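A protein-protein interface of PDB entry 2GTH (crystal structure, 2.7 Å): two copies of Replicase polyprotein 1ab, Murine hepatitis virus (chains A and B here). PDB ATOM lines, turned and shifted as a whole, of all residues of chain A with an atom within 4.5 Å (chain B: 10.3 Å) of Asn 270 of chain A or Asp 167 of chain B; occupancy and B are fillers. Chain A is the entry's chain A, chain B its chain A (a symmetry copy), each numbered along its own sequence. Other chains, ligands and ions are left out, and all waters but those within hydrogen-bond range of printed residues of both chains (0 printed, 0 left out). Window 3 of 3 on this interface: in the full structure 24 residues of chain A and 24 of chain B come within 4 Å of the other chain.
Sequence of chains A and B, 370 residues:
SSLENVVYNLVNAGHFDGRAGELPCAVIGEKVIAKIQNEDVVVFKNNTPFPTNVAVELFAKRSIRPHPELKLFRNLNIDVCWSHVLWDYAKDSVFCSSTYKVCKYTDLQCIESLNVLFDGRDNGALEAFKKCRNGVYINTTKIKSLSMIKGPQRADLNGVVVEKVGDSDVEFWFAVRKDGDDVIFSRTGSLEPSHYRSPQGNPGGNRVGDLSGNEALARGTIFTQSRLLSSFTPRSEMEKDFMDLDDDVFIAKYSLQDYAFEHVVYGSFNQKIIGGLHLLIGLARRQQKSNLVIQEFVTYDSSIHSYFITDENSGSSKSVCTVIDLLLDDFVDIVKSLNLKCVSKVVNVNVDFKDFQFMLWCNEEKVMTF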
ATOM      1  N   SER A 268      23.685  29.863  35.234  1.00  0.00           N
ATOM      2  CA  SER A 268      23.335  29.344  33.924  1.00  0.00           C
ATOM      3  C   SER A 268      24.152  28.094  33.597  1.00  0.00           C
ATOM      4  O   SER A 268      25.368  28.079  33.746  1.00  0.00           O
ATOM      5  CB  SER A 268      23.533  30.417  32.851  1.00  0.00           C
ATOM      6  OG  SER A 268      24.796  31.044  32.951  1.00  0.00           O
ATOM      7  N   PHE A 269      23.477  27.052  33.125  1.00  0.00           N
ATOM      8  CA  PHE A 269      24.127  25.791  32.825  1.00  0.00           C
ATOM      9  C   PHE A 269      24.145  25.358  31.357  1.00  0.00           C
ATOM     10  O   PHE A 269      24.382  24.198  31.054  1.00  0.00           O
ATOM     11  CB  PHE A 269      23.455  24.730  33.673  1.00  0.00           C
ATOM     12  CG  PHE A 269      23.524  25.010  35.143  1.00  0.00           C
ATOM     13  CD1 PHE A 269      24.691  24.742  35.864  1.00  0.00           C
ATOM     14  CD2 PHE A 269      22.433  25.539  35.814  1.00  0.00           C
ATOM     15  CE1 PHE A 269      24.762  25.001  37.240  1.00  0.00           C
ATOM     16  CE2 PHE A 269      22.501  25.798  37.180  1.00  0.00           C
ATOM     17  CZ  PHE A 269      23.666  25.529  37.895  1.00  0.00           C
ATOM     18  N   ASN A 270      23.910  26.295  30.453  1.00  0.00           N
ATOM     19  CA  ASN A 270      23.874  26.002  29.028  1.00  0.00           C
ATOM     20  C   ASN A 270      25.206  25.945  28.328  1.00  0.00           C
ATOM     21  O   ASN A 270      25.308  25.417  27.232  1.00  0.00           O
ATOM     22  CB  ASN A 270      23.023  27.028  28.319  1.00  0.00           C
ATOM     23  CG  ASN A 270      21.585  26.881  28.661  1.00  0.00           C
ATOM     24  OD1 ASN A 270      20.725  27.572  28.112  1.00  0.00           O
ATOM     25  ND2 ASN A 270      21.296  25.960  29.579  1.00  0.00           N
ATOM     26  N   GLN A 271      26.226  26.514  28.932  1.00  0.00           N
ATOM     27  CA  GLN A 271      27.511  26.493  28.303  1.00  0.00           C
ATOM     28  C   GLN A 271      28.312  25.420  28.979  1.00  0.00           C
ATOM     29  O   GLN A 271      27.771  24.611  29.723  1.00  0.00           O
ATOM     30  CB  GLN A 271      28.204  27.841  28.469  1.00  0.00           C
ATOM     31  CG  GLN A 271      27.275  29.013  28.320  1.00  0.00           C
ATOM     32  CD  GLN A 271      26.440  29.253  29.564  1.00  0.00           C
ATOM     33  OE1 GLN A 271      25.243  29.533  29.465  1.00  0.00           O
ATOM     34  NE2 GLN A 271      27.066  29.161  30.743  1.00  0.00           N
ATOM     35  N   LYS A 272      29.608  25.429  28.712  1.00  0.00           N
ATOM     36  CA  LYS A 272      30.516  24.475  29.303  1.00  0.00           C
ATOM     37  C   LYS A 272      30.936  25.052  30.640  1.00  0.00           C
ATOM     38  O   LYS A 272      31.224  24.312  31.578  1.00  0.00           O
ATOM     39  CB  LYS A 272      31.726  24.263  28.386  1.00  0.00           C
ATOM     40  CG  LYS A 272      31.398  23.422  27.169  1.00  0.00           C
ATOM     41  CD  LYS A 272      32.526  23.399  26.168  1.00  0.00           C
ATOM     42  CE  LYS A 272      33.827  22.905  26.789  1.00  0.00           C
ATOM     43  NZ  LYS A 272      34.961  22.893  25.802  1.00  0.00           N
ATOM     44  N   SER A 314      23.747  18.930  33.400  1.00  0.00           N
ATOM     45  CA  SER A 314      24.060  19.651  32.163  1.00  0.00           C
ATOM     46  C   SER A 314      25.474  19.466  31.689  1.00  0.00           C
ATOM     47  O   SER A 314      25.801  19.800  30.543  1.00  0.00           O
ATOM     48  CB  SER A 314      23.794  21.145  32.333  1.00  0.00           C
ATOM     49  OG  SER A 314      24.697  21.700  33.272  1.00  0.00           O
ATOM     50  N   PRO B  66      35.667  16.822  29.922  1.00  0.00           N
ATOM     51  CA  PRO B  66      35.001  15.520  29.843  1.00  0.00           C
ATOM     52  C   PRO B  66      35.781  14.506  29.033  1.00  0.00           C
ATOM     53  O   PRO B  66      36.561  14.872  28.165  1.00  0.00           O
ATOM     54  CB  PRO B  66      33.676  15.853  29.174  1.00  0.00           C
ATOM     55  CG  PRO B  66      33.484  17.311  29.423  1.00  0.00           C
ATOM     56  CD  PRO B  66      34.866  17.853  29.246  1.00  0.00           C
ATOM     57  N   LEU B 157      33.229  13.431  33.881  1.00  0.00           N
ATOM     58  CA  LEU B 157      33.587  14.853  33.968  1.00  0.00           C
ATOM     59  C   LEU B 157      33.914  15.115  35.418  1.00  0.00           C
ATOM     60  O   LEU B 157      33.011  15.304  36.222  1.00  0.00           O
ATOM     61  CB  LEU B 157      32.445  15.784  33.558  1.00  0.00           C
ATOM     62  CG  LEU B 157      32.764  17.280  33.759  1.00  0.00           C
ATOM     63  CD1 LEU B 157      34.064  17.680  33.023  1.00  0.00           C
ATOM     64  CD2 LEU B 157      31.604  18.106  33.268  1.00  0.00           C
ATOM     65  N   VAL B 162      28.210  12.436  33.262  1.00  0.00           N
ATOM     66  CA  VAL B 162      27.270  13.346  32.618  1.00  0.00           C
ATOM     67  C   VAL B 162      26.825  12.813  31.258  1.00  0.00           C
ATOM     68  O   VAL B 162      27.491  11.957  30.675  1.00  0.00           O
ATOM     69  CB  VAL B 162      27.910  14.748  32.473  1.00  0.00           C
ATOM     70  CG1 VAL B 162      28.577  15.126  33.800  1.00  0.00           C
ATOM     71  CG2 VAL B 162      28.945  14.765  31.349  1.00  0.00           C
ATOM     72  N   GLU B 163      25.692  13.313  30.762  1.00  0.00           N
ATOM     73  CA  GLU B 163      25.147  12.877  29.475  1.00  0.00           C
ATOM     74  C   GLU B 163      24.989  14.065  28.553  1.00  0.00           C
ATOM     75  O   GLU B 163      24.531  13.949  27.418  1.00  0.00           O
ATOM     76  CB  GLU B 163      23.811  12.192  29.689  1.00  0.00           C
ATOM     77  CG  GLU B 163      23.873  11.221  30.837  1.00  0.00           C
ATOM     78  CD  GLU B 163      22.720  10.252  30.857  1.00  0.00           C
ATOM     79  OE1 GLU B 163      21.575  10.690  30.572  1.00  0.00           O
ATOM     80  OE2 GLU B 163      22.966   9.054  31.172  1.00  0.00           O
ATOM     81  N   LYS B 164      25.399  15.209  29.072  1.00  0.00           N
ATOM     82  CA  LYS B 164      25.355  16.458  28.354  1.00  0.00           C
ATOM     83  C   LYS B 164      26.511  17.296  28.868  1.00  0.00           C
ATOM     84  O   LYS B 164      27.007  17.064  29.970  1.00  0.00           O
ATOM     85  CB  LYS B 164      24.058  17.222  28.639  1.00  0.00           C
ATOM     86  CG  LYS B 164      22.821  16.662  28.012  1.00  0.00           C
ATOM     87  CD  LYS B 164      21.669  17.611  28.200  1.00  0.00           C
ATOM     88  CE  LYS B 164      20.400  17.072  27.563  1.00  0.00           C
ATOM     89  NZ  LYS B 164      20.058  15.723  28.089  1.00  0.00           N
ATOM     90  N   VAL B 165      26.932  18.264  28.063  1.00  0.00           N
ATOM     91  CA  VAL B 165      27.983  19.178  28.450  1.00  0.00           C
ATOM     92  C   VAL B 165      27.533  20.519  27.910  1.00  0.00           C
ATOM     93  O   VAL B 165      27.804  20.872  26.760  1.00  0.00           O
ATOM     94  CB  VAL B 165      29.337  18.781  27.854  1.00  0.00           C
ATOM     95  CG1 VAL B 165      30.387  19.812  28.234  1.00  0.00           C
ATOM     96  CG2 VAL B 165      29.747  17.424  28.377  1.00  0.00           C
ATOM     97  N   GLY B 166      26.825  21.264  28.752  1.00  0.00           N
ATOM     98  CA  GLY B 166      26.300  22.550  28.329  1.00  0.00           C
ATOM     99  C   GLY B 166      25.035  22.201  27.580  1.00  0.00           C
ATOM    100  O   GLY B 166      24.773  22.697  26.483  1.00  0.00           O
ATOM    101  N   ASP B 167      24.268  21.299  28.188  1.00  0.00           N
ATOM    102  CA  ASP B 167      23.021  20.803  27.630  1.00  0.00           C
ATOM    103  C   ASP B 167      23.149  20.191  26.247  1.00  0.00           C
ATOM    104  O   ASP B 167      22.151  19.879  25.598  1.00  0.00           O
ATOM    105  CB  ASP B 167      21.979  21.905  27.631  1.00  0.00           C
ATOM    106  CG  ASP B 167      21.650  22.343  29.014  1.00  0.00           C
ATOM    107  OD1 ASP B 167      21.609  21.447  29.892  1.00  0.00           O
ATOM    108  OD2 ASP B 167      21.441  23.561  29.232  1.00  0.00           O
ATOM    109  N   SER B 168      24.383  20.045  25.787  1.00  0.00           N
ATOM    110  CA  SER B 168      24.626  19.412  24.515  1.00  0.00           C
ATOM    111  C   SER B 168      25.080  18.015  24.862  1.00  0.00           C
ATOM    112  O   SER B 168      25.935  17.819  25.733  1.00  0.00           O
ATOM    113  CB  SER B 168      25.701  20.138  23.716  1.00  0.00           C
ATOM    114  OG  SER B 168      25.190  21.351  23.220  1.00  0.00           O
ATOM    115  N   ASP B 169      24.478  17.045  24.192  1.00  0.00           N
ATOM    116  CA  ASP B 169      24.791  15.656  24.413  1.00  0.00           C
ATOM    117  C   ASP B 169      26.262  15.312  24.288  1.00  0.00           C
ATOM    118  O   ASP B 169      27.003  15.903  23.503  1.00  0.00           O
ATOM    119  CB  ASP B 169      23.992  14.814  23.446  1.00  0.00           C
ATOM    120  CG  ASP B 169      22.535  14.939  23.676  1.00  0.00           C
ATOM    121  OD1 ASP B 169      22.089  14.624  24.802  1.00  0.00           O
ATOM    122  OD2 ASP B 169      21.837  15.358  22.736  1.00  0.00           O
ATOM    123  N   VAL B 170      26.673  14.340  25.081  1.00  0.00           N
ATOM    124  CA  VAL B 170      28.039  13.894  25.060  1.00  0.00           C
ATOM    125  C   VAL B 170      28.235  13.057  23.819  1.00  0.00           C
ATOM    126  O   VAL B 170      27.401  12.222  23.494  1.00  0.00           O
ATOM    127  CB  VAL B 170      28.347  13.029  26.279  1.00  0.00           C
ATOM    128  CG1 VAL B 170      29.699  12.355  26.098  1.00  0.00           C
ATOM    129  CG2 VAL B 170      28.325  13.885  27.549  1.00  0.00           C
ATOM    130  N   GLU B 171      29.336  13.277  23.111  1.00  0.00           N
ATOM    131  CA  GLU B 171      29.616  12.493  21.910  1.00  0.00           C
ATOM    132  C   GLU B 171      31.094  12.175  21.839  1.00  0.00           C
ATOM    133  O   GLU B 171      31.924  13.043  22.070  1.00  0.00           O
ATOM    134  CB  GLU B 171      29.196  13.263  20.666  1.00  0.00           C
ATOM    135  CG  GLU B 171      29.784  12.712  19.385  1.00  0.00           C
ATOM    136  CD  GLU B 171      29.215  13.389  18.147  1.00  0.00           C
ATOM    137  OE1 GLU B 171      29.182  14.643  18.094  1.00  0.00           O
ATOM    138  OE2 GLU B 171      28.798  12.662  17.218  1.00  0.00           O
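Of the 12 printed residues of chain B, 4 touch a printed residue of chain A.
Along chain B the printed residues that touch a printed residue of chain A span positions 164 to 167.
Of the 6 printed residues of chain A, 5 touch a printed residue of chain B.
Printed residues of chain A that touch a printed residue of chain B: Phe 269, Asn 270, Gln 271, Lys 272 and Ser 314.
No position is printed for both chains.
Of the 10 pairs that touch across the chains among the printed residues, none has its exchanged pair printed and touching as well.
Asn 270 of chain A touches two residues of chain B.
Asp 167 of chain B touches just these residues of chain A: Phe 269, Asn 270 and Ser 314.
Gln 271 of chain A touches just one residue of chain B: Gly 166.
Of chain B, only Lys 164, Val 165, Gly 166 and Asp 167 come within 4 Å of Ser 314 of chain A.
Printed residues of chain B within 4 Å of Lys 272 of chain A: Val 165 (3.9 Å).
Printed residues of chain A within 4 Å of Lys 164 of chain B: Ser 314.
Of the printed residues of chain A, Val 165 of chain B touches Lys 272 (3.9 Å) and Ser 314 (3.1 Å).
The nearest residue of chain B that does not touch Asn 270 of chain A is Val 165 of chain B (5.2 Å).
The nearest printed residue of chain A that does not touch Asp 167 of chain B is Gln 271 of chain A (5.1 Å).
Among the printed residues, merely in contact across the chains: Phe 269 of chain A with Gly 166 of chain B, Phe 269 of chain A with Asp 167 of chain B, Gln 271 of chain A with Gly 166 of chain B and Lys 272 of chain A with Val 165 of chain B.
The backbone carbonyl oxygen of Asn 270 of chain A sits close to the backbone carbonyl oxygen of Gly 166 of chain B, 2.9 Å away.
O of Ser 314 of chain A sits at hydrogen-bond distance from N of Asp 167 of chain B, 3.2 Å away.
The backbone NH (N) of Val 165 of chain B sits close to the backbone carbonyl oxygen (O) of Ser 314 of chain A (3.1 Å).
The side-chain amide nitrogen (ND2) of Asn 270 of chain A lies within hydrogen-bond range of the side-chain carboxylate (OD2) of Asp 167 of chain B (2.4 Å).
The backbone carbonyl oxygen (O) of Ser 314 of chain A lies close to the backbone carbonyl oxygen (O) of Lys 164 of chain B, at 3.0 Å.
N of Gly 166 of chain B sits at hydrogen-bond distance from O of Ser 314 of chain A, 2.5 Å away.
O of Phe 269 of chain A lies close to OG of Ser 314 of chain A (3.4 Å).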
